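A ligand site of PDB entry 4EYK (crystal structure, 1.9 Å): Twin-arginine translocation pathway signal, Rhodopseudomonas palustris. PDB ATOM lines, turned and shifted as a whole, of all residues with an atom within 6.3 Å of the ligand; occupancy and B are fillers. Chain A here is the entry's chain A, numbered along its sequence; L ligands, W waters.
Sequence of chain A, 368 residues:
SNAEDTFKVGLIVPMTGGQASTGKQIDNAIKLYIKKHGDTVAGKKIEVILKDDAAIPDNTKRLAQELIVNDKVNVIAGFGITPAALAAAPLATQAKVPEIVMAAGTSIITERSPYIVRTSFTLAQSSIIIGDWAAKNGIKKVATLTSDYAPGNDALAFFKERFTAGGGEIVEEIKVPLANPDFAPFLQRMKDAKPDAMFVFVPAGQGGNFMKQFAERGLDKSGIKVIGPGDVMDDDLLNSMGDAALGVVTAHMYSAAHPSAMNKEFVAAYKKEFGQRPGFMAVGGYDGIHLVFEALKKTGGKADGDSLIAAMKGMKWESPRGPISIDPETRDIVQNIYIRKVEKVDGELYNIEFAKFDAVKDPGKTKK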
ATOM      1  N   GLN A  19     -21.957   3.482 -19.122  1.00  0.00           N
ATOM      2  CA  GLN A  19     -22.976   2.722 -19.830  1.00  0.00           C
ATOM      3  C   GLN A  19     -23.579   1.603 -18.985  1.00  0.00           C
ATOM      4  O   GLN A  19     -24.074   0.629 -19.551  1.00  0.00           O
ATOM      5  CB  GLN A  19     -22.441   2.181 -21.167  1.00  0.00           C
ATOM      6  CG  GLN A  19     -21.797   3.247 -22.041  1.00  0.00           C
ATOM      7  CD  GLN A  19     -22.720   4.426 -22.283  1.00  0.00           C
ATOM      8  OE1 GLN A  19     -22.439   5.555 -21.872  1.00  0.00           O
ATOM      9  NE2 GLN A  19     -23.844   4.164 -22.954  1.00  0.00           N
ATOM     10  N   THR A  22     -27.050   0.059 -19.871  1.00  0.00           N
ATOM     11  CA  THR A  22     -27.091  -0.906 -20.976  1.00  0.00           C
ATOM     12  C   THR A  22     -26.961  -2.331 -20.450  1.00  0.00           C
ATOM     13  O   THR A  22     -27.802  -3.193 -20.747  1.00  0.00           O
ATOM     14  CB  THR A  22     -26.005  -0.584 -22.025  1.00  0.00           C
ATOM     15  OG1 THR A  22     -26.287   0.693 -22.610  1.00  0.00           O
ATOM     16  CG2 THR A  22     -25.952  -1.637 -23.128  1.00  0.00           C
ATOM     17  N   GLY A  80     -21.796  -3.653 -25.244  1.00  0.00           N
ATOM     18  CA  GLY A  80     -22.595  -2.474 -24.929  1.00  0.00           C
ATOM     19  C   GLY A  80     -22.301  -1.247 -25.759  1.00  0.00           C
ATOM     20  O   GLY A  80     -23.140  -0.362 -25.870  1.00  0.00           O
ATOM     21  N   ILE A  81     -21.082  -1.173 -26.306  1.00  0.00           N
ATOM     22  CA  ILE A  81     -20.671  -0.076 -27.200  1.00  0.00           C
ATOM     23  C   ILE A  81     -19.901  -0.668 -28.388  1.00  0.00           C
ATOM     24  O   ILE A  81     -19.419  -1.812 -28.319  1.00  0.00           O
ATOM     25  CB  ILE A  81     -19.845   1.042 -26.488  1.00  0.00           C
ATOM     26  CG1 ILE A  81     -18.498   0.514 -25.931  1.00  0.00           C
ATOM     27  CG2 ILE A  81     -20.633   1.686 -25.345  1.00  0.00           C
ATOM     28  CD1 ILE A  81     -17.533   1.655 -25.614  1.00  0.00           C
ATOM     29  N   THR A  82     -19.811   0.097 -29.481  1.00  0.00           N
ATOM     30  CA  THR A  82     -19.175  -0.388 -30.708  1.00  0.00           C
ATOM     31  C   THR A  82     -17.734  -0.894 -30.495  1.00  0.00           C
ATOM     32  O   THR A  82     -17.402  -2.009 -30.904  1.00  0.00           O
ATOM     33  CB  THR A  82     -19.279   0.685 -31.820  1.00  0.00           C
ATOM     34  OG1 THR A  82     -20.643   0.788 -32.283  1.00  0.00           O
ATOM     35  CG2 THR A  82     -18.367   0.345 -32.986  1.00  0.00           C
ATOM     36  N   PRO A  83     -16.875  -0.103 -29.816  1.00  0.00           N
ATOM     37  CA  PRO A  83     -15.511  -0.604 -29.549  1.00  0.00           C
ATOM     38  C   PRO A  83     -15.473  -1.976 -28.852  1.00  0.00           C
ATOM     39  O   PRO A  83     -14.539  -2.747 -29.093  1.00  0.00           O
ATOM     40  CB  PRO A  83     -14.919   0.464 -28.630  1.00  0.00           C
ATOM     41  CG  PRO A  83     -15.616   1.721 -29.062  1.00  0.00           C
ATOM     42  CD  PRO A  83     -17.031   1.296 -29.366  1.00  0.00           C
ATOM     43  N   ALA A 103     -26.474  -4.708 -28.365  1.00  0.00           N
ATOM     44  CA  ALA A 103     -26.501  -3.278 -28.066  1.00  0.00           C
ATOM     45  C   ALA A 103     -25.871  -2.447 -29.179  1.00  0.00           C
ATOM     46  O   ALA A 103     -26.571  -1.649 -29.807  1.00  0.00           O
ATOM     47  CB  ALA A 103     -25.824  -3.004 -26.727  1.00  0.00           C
ATOM     48  N   ALA A 104     -24.575  -2.658 -29.451  1.00  0.00           N
ATOM     49  CA  ALA A 104     -23.809  -1.756 -30.337  1.00  0.00           C
ATOM     50  C   ALA A 104     -24.451  -1.585 -31.723  1.00  0.00           C
ATOM     51  O   ALA A 104     -24.948  -2.556 -32.320  1.00  0.00           O
ATOM     52  CB  ALA A 104     -22.364  -2.212 -30.461  1.00  0.00           C
ATOM     53  N   GLY A 105     -24.410  -0.360 -32.240  1.00  0.00           N
ATOM     54  CA  GLY A 105     -25.217   0.013 -33.409  1.00  0.00           C
ATOM     55  C   GLY A 105     -24.506   0.531 -34.641  1.00  0.00           C
ATOM     56  O   GLY A 105     -25.151   1.095 -35.527  1.00  0.00           O
ATOM     57  N   THR A 106     -23.186   0.349 -34.738  1.00  0.00           N
ATOM     58  CA  THR A 106     -22.433   0.828 -35.913  1.00  0.00           C
ATOM     59  C   THR A 106     -22.616  -0.164 -37.056  1.00  0.00           C
ATOM     60  O   THR A 106     -22.533  -1.376 -36.841  1.00  0.00           O
ATOM     61  CB  THR A 106     -20.957   1.063 -35.542  1.00  0.00           C
ATOM     62  OG1 THR A 106     -20.917   2.100 -34.565  1.00  0.00           O
ATOM     63  CG2 THR A 106     -20.114   1.485 -36.735  1.00  0.00           C
ATOM     64  N   ILE A 109     -20.084  -3.247 -37.991  1.00  0.00           N
ATOM     65  CA  ILE A 109     -19.807  -4.295 -37.007  1.00  0.00           C
ATOM     66  C   ILE A 109     -19.984  -5.734 -37.534  1.00  0.00           C
ATOM     67  O   ILE A 109     -19.121  -6.584 -37.325  1.00  0.00           O
ATOM     68  CB  ILE A 109     -20.607  -4.082 -35.707  1.00  0.00           C
ATOM     69  CG1 ILE A 109     -20.116  -2.818 -35.001  1.00  0.00           C
ATOM     70  CG2 ILE A 109     -20.483  -5.298 -34.792  1.00  0.00           C
ATOM     71  CD1 ILE A 109     -20.918  -2.469 -33.752  1.00  0.00           C
ATOM     72  N   PHE A 121     -29.701  -3.005 -33.526  1.00  0.00           N
ATOM     73  CA  PHE A 121     -30.091  -2.010 -34.540  1.00  0.00           C
ATOM     74  C   PHE A 121     -28.828  -1.494 -35.191  1.00  0.00           C
ATOM     75  O   PHE A 121     -27.710  -1.765 -34.705  1.00  0.00           O
ATOM     76  CB  PHE A 121     -30.812  -0.788 -33.888  1.00  0.00           C
ATOM     77  CG  PHE A 121     -30.077  -0.231 -32.685  1.00  0.00           C
ATOM     78  CD1 PHE A 121     -29.027   0.669 -32.845  1.00  0.00           C
ATOM     79  CD2 PHE A 121     -30.407  -0.651 -31.395  1.00  0.00           C
ATOM     80  CE1 PHE A 121     -28.317   1.149 -31.732  1.00  0.00           C
ATOM     81  CE2 PHE A 121     -29.717  -0.183 -30.284  1.00  0.00           C
ATOM     82  CZ  PHE A 121     -28.669   0.726 -30.442  1.00  0.00           C
ATOM     83  N   LEU A 123     -27.538   2.532 -36.326  1.00  0.00           N
ATOM     84  CA  LEU A 123     -27.929   3.942 -36.275  1.00  0.00           C
ATOM     85  C   LEU A 123     -28.469   4.377 -37.621  1.00  0.00           C
ATOM     86  O   LEU A 123     -29.397   5.184 -37.663  1.00  0.00           O
ATOM     87  CB  LEU A 123     -26.759   4.838 -35.834  1.00  0.00           C
ATOM     88  CG  LEU A 123     -26.796   5.222 -34.342  1.00  0.00           C
ATOM     89  CD1 LEU A 123     -28.068   6.029 -34.000  1.00  0.00           C
ATOM     90  CD2 LEU A 123     -26.675   3.977 -33.448  1.00  0.00           C
ATOM     91  N   TYR A 149     -17.991   9.215 -31.466  1.00  0.00           N
ATOM     92  CA  TYR A 149     -17.409   7.928 -31.822  1.00  0.00           C
ATOM     93  C   TYR A 149     -18.289   7.256 -32.869  1.00  0.00           C
ATOM     94  O   TYR A 149     -19.279   7.855 -33.303  1.00  0.00           O
ATOM     95  CB  TYR A 149     -17.141   7.049 -30.579  1.00  0.00           C
ATOM     96  CG  TYR A 149     -18.347   6.397 -29.902  1.00  0.00           C
ATOM     97  CD1 TYR A 149     -18.407   5.009 -29.761  1.00  0.00           C
ATOM     98  CD2 TYR A 149     -19.396   7.169 -29.383  1.00  0.00           C
ATOM     99  CE1 TYR A 149     -19.489   4.409 -29.135  1.00  0.00           C
ATOM    100  CE2 TYR A 149     -20.484   6.579 -28.765  1.00  0.00           C
ATOM    101  CZ  TYR A 149     -20.531   5.204 -28.640  1.00  0.00           C
ATOM    102  OH  TYR A 149     -21.612   4.624 -28.003  1.00  0.00           O
ATOM    103  N   ALA A 150     -17.909   6.060 -33.300  1.00  0.00           N
ATOM    104  CA  ALA A 150     -18.517   5.416 -34.472  1.00  0.00           C
ATOM    105  C   ALA A 150     -20.056   5.544 -34.686  1.00  0.00           C
ATOM    106  O   ALA A 150     -20.475   6.003 -35.757  1.00  0.00           O
ATOM    107  CB  ALA A 150     -18.069   3.959 -34.591  1.00  0.00           C
ATOM    108  N   PRO A 151     -20.890   5.131 -33.703  1.00  0.00           N
ATOM    109  CA  PRO A 151     -22.343   5.184 -33.978  1.00  0.00           C
ATOM    110  C   PRO A 151     -22.843   6.619 -34.152  1.00  0.00           C
ATOM    111  O   PRO A 151     -23.818   6.860 -34.885  1.00  0.00           O
ATOM    112  CB  PRO A 151     -22.962   4.534 -32.712  1.00  0.00           C
ATOM    113  CG  PRO A 151     -21.941   4.789 -31.661  1.00  0.00           C
ATOM    114  CD  PRO A 151     -20.638   4.585 -32.358  1.00  0.00           C
ATOM    115  N   LEU A 178     -17.956  10.417 -25.551  1.00  0.00           N
ATOM    116  CA  LEU A 178     -18.726   9.326 -24.961  1.00  0.00           C
ATOM    117  C   LEU A 178     -18.724   9.428 -23.417  1.00  0.00           C
ATOM    118  O   LEU A 178     -19.789   9.336 -22.774  1.00  0.00           O
ATOM    119  CB  LEU A 178     -18.176   7.963 -25.425  1.00  0.00           C
ATOM    120  CG  LEU A 178     -18.726   6.704 -24.748  1.00  0.00           C
ATOM    121  CD1 LEU A 178     -20.236   6.583 -24.970  1.00  0.00           C
ATOM    122  CD2 LEU A 178     -18.025   5.435 -25.230  1.00  0.00           C
ATOM    123  N   PHE A 201     -27.832  12.622 -31.199  1.00  0.00           N
ATOM    124  CA  PHE A 201     -27.562  11.250 -30.839  1.00  0.00           C
ATOM    125  C   PHE A 201     -26.681  11.238 -29.605  1.00  0.00           C
ATOM    126  O   PHE A 201     -25.581  11.818 -29.620  1.00  0.00           O
ATOM    127  CB  PHE A 201     -26.862  10.430 -31.950  1.00  0.00           C
ATOM    128  CG  PHE A 201     -26.308   9.126 -31.436  1.00  0.00           C
ATOM    129  CD1 PHE A 201     -27.153   8.051 -31.151  1.00  0.00           C
ATOM    130  CD2 PHE A 201     -24.938   8.997 -31.129  1.00  0.00           C
ATOM    131  CE1 PHE A 201     -26.657   6.859 -30.621  1.00  0.00           C
ATOM    132  CE2 PHE A 201     -24.433   7.806 -30.603  1.00  0.00           C
ATOM    133  CZ  PHE A 201     -25.291   6.742 -30.344  1.00  0.00           C
ATOM    134  N   VAL A 202     -27.159  10.594 -28.550  1.00  0.00           N
ATOM    135  CA  VAL A 202     -26.305  10.232 -27.422  1.00  0.00           C
ATOM    136  C   VAL A 202     -26.695   8.784 -27.122  1.00  0.00           C
ATOM    137  O   VAL A 202     -27.829   8.386 -27.402  1.00  0.00           O
ATOM    138  CB  VAL A 202     -26.499  11.153 -26.187  1.00  0.00           C
ATOM    139  CG1 VAL A 202     -26.017  12.583 -26.483  1.00  0.00           C
ATOM    140  CG2 VAL A 202     -27.951  11.161 -25.692  1.00  0.00           C
ATOM    141  N   PRO A 203     -25.749   7.989 -26.587  1.00  0.00           N
ATOM    142  CA  PRO A 203     -26.050   6.559 -26.357  1.00  0.00           C
ATOM    143  C   PRO A 203     -27.043   6.344 -25.225  1.00  0.00           C
ATOM    144  O   PRO A 203     -27.299   7.266 -24.452  1.00  0.00           O
ATOM    145  CB  PRO A 203     -24.680   5.976 -25.952  1.00  0.00           C
ATOM    146  CG  PRO A 203     -23.922   7.150 -25.406  1.00  0.00           C
ATOM    147  CD  PRO A 203     -24.351   8.318 -26.258  1.00  0.00           C
ATOM    148  N   ALA A 204     -27.622   5.142 -25.143  1.00  0.00           N
ATOM    149  CA  ALA A 204     -28.460   4.745 -24.006  1.00  0.00           C
ATOM    150  C   ALA A 204     -27.820   5.209 -22.701  1.00  0.00           C
ATOM    151  O   ALA A 204     -26.604   5.102 -22.544  1.00  0.00           O
ATOM    152  CB  ALA A 204     -28.639   3.229 -23.992  1.00  0.00           C
ATOM    153  N   GLY A 205     -28.636   5.758 -21.798  1.00  0.00           N
ATOM    154  CA  GLY A 205     -28.163   6.147 -20.478  1.00  0.00           C
ATOM    155  C   GLY A 205     -27.879   7.633 -20.331  1.00  0.00           C
ATOM    156  O   GLY A 205     -27.763   8.131 -19.215  1.00  0.00           O
ATOM    157  N   ASP A 231     -32.364   6.870 -29.402  1.00  0.00           N
ATOM    158  CA  ASP A 231     -31.452   6.617 -28.273  1.00  0.00           C
ATOM    159  C   ASP A 231     -31.594   7.669 -27.175  1.00  0.00           C
ATOM    160  O   ASP A 231     -31.643   7.328 -25.991  1.00  0.00           O
ATOM    161  CB  ASP A 231     -30.007   6.527 -28.768  1.00  0.00           C
ATOM    162  CG  ASP A 231     -29.872   5.572 -29.947  1.00  0.00           C
ATOM    163  OD1 ASP A 231     -29.323   4.465 -29.730  1.00  0.00           O
ATOM    164  OD2 ASP A 231     -30.345   5.926 -31.062  1.00  0.00           O
ATOM    165  N   HIS A 252     -37.119   5.086 -34.193  1.00  0.00           N
ATOM    166  CA  HIS A 252     -36.382   4.018 -33.534  1.00  0.00           C
ATOM    167  C   HIS A 252     -37.046   2.696 -33.733  1.00  0.00           C
ATOM    168  O   HIS A 252     -38.185   2.625 -34.176  1.00  0.00           O
ATOM    169  CB  HIS A 252     -36.253   4.312 -32.027  1.00  0.00           C
ATOM    170  CG  HIS A 252     -34.923   3.902 -31.460  1.00  0.00           C
ATOM    171  ND1 HIS A 252     -34.711   3.737 -30.131  1.00  0.00           N
ATOM    172  CD2 HIS A 252     -33.705   3.619 -32.081  1.00  0.00           C
ATOM    173  CE1 HIS A 252     -33.426   3.381 -29.913  1.00  0.00           C
ATOM    174  NE2 HIS A 252     -32.812   3.286 -31.110  1.00  0.00           N
ATOM    175  N   PHE A 280     -34.955   0.183 -24.985  1.00  0.00           N
ATOM    176  CA  PHE A 280     -34.564  -0.500 -26.200  1.00  0.00           C
ATOM    177  C   PHE A 280     -33.357  -1.429 -26.040  1.00  0.00           C
ATOM    178  O   PHE A 280     -33.192  -2.384 -26.809  1.00  0.00           O
ATOM    179  CB  PHE A 280     -34.363   0.508 -27.345  1.00  0.00           C
ATOM    180  CG  PHE A 280     -33.192   1.425 -27.153  1.00  0.00           C
ATOM    181  CD1 PHE A 280     -31.922   1.075 -27.624  1.00  0.00           C
ATOM    182  CD2 PHE A 280     -33.353   2.654 -26.499  1.00  0.00           C
ATOM    183  CE1 PHE A 280     -30.840   1.932 -27.461  1.00  0.00           C
ATOM    184  CE2 PHE A 280     -32.263   3.522 -26.339  1.00  0.00           C
ATOM    185  CZ  PHE A 280     -31.018   3.159 -26.821  1.00  0.00           C
ATOM    186  N   MET A 281     -32.493  -1.180 -25.052  1.00  0.00           N
ATOM    187  CA  MET A 281     -31.398  -2.133 -24.802  1.00  0.00           C
ATOM    188  C   MET A 281     -31.900  -3.458 -24.223  1.00  0.00           C
ATOM    189  O   MET A 281     -31.372  -4.533 -24.540  1.00  0.00           O
ATOM    190  CB  MET A 281     -30.292  -1.507 -23.918  1.00  0.00           C
ATOM    191  CG  MET A 281     -29.570  -0.380 -24.660  1.00  0.00           C
ATOM    192  SD  MET A 281     -28.799  -1.033 -26.318  1.00  0.00           S
ATOM    193  CE  MET A 281     -27.476   0.356 -26.537  1.00  0.00           C
HETATM  194  C1  LIG L   1     -24.063   2.424 -29.272  1.00  0.00           C
HETATM  195  C2  LIG L   1     -24.270   2.479 -27.880  1.00  0.00           C
HETATM  196  C3  LIG L   1     -25.497   2.947 -27.414  1.00  0.00           C
HETATM  197  O1  LIG L   1     -25.779   3.027 -26.087  1.00  0.00           O
HETATM  198  C4  LIG L   1     -26.532   3.361 -28.377  1.00  0.00           C
HETATM  199  O2  LIG L   1     -27.718   3.811 -27.874  1.00  0.00           O
HETATM  200  C5  LIG L   1     -26.302   3.287 -29.747  1.00  0.00           C
HETATM  201  C6  LIG L   1     -25.057   2.811 -30.199  1.00  0.00           C
HETATM  202  C7  LIG L   1     -22.750   1.941 -29.775  1.00  0.00           C
HETATM  203  O3  LIG L   1     -22.710   1.436 -30.914  1.00  0.00           O
HETATM  204  O4  LIG L   1     -21.727   2.083 -29.053  1.00  0.00           O
HETATM  205  O   HOH W   1     -24.384   1.575 -24.358  1.00  0.00           O
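An oxygen (O2) of the ligand sits at hydrogen-bond distance from the side-chain carboxylate (OD1) of Asp 231, at 2.5 Å.
N of Thr 82 lies within hydrogen-bond range of O4 of the ligand, at 2.8 Å.
An oxygen (O3) of the ligand is in hydrogen-bond range of the side-chain hydroxyl (OG1) of Thr 82 (2.6 Å).
OH of Tyr 149 is in hydrogen-bond range of O4 of the ligand, at 2.8 Å.
The backbone NH of Gly 105 sits at hydrogen-bond distance from an oxygen (O3) of the ligand, 2.8 Å away.
The backbone NH (N) of Ala 204 lies within hydrogen-bond range of an oxygen (O1) of the ligand (3.0 Å).
Water W1 lies within hydrogen-bond range of O1 of the ligand, OG1 of Thr 22, O of Gly 80 and NE2 of Gln 19.
NE2 of Gln 19 touches O1 of the ligand (3.9 Å).
O of Gly 80 touches C2 of the ligand, at 3.7 Å.
Ile 81 touches the ligand (CA to O4, 3.0 Å).
Ala 104 touches the ligand.
Phe 121 touches the ligand.
Leu 123 touches the ligand.
CG of Pro 151 touches C7 of the ligand (3.5 Å).
Phe 201 touches the ligand.
Pro 203 touches the ligand (CB to O1, 3.2 Å).
CZ of Phe 280 touches O2 of the ligand, at 3.5 Å.
CE of Met 281 touches O1 of the ligand (3.2 Å).
Hydrophobic or aromatic side chains that line the ligand: Ile 81, Ala 104, Phe 121, Leu 123, Tyr 149, Pro 151, Phe 201, Pro 203, Ala 204, Phe 280 and Met 281.
Of the 26 residues printed, 16 come within 4 Å of the ligand.
Along chain A the residues within 4 Å of the ligand span positions 19 to 281.
OG1 of Thr 82 sits at hydrogen-bond distance from OG1 of Thr 106, 2.6 Å away.
The backbone carbonyl oxygen of Gly 105 is in hydrogen-bond range of the backbone NH of Leu 123, 2.9 Å away.
The backbone carbonyl oxygen (O) of Ala 204 sits at hydrogen-bond distance from the side-chain amide nitrogen (NE2) of Gln 19 (2.9 Å).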
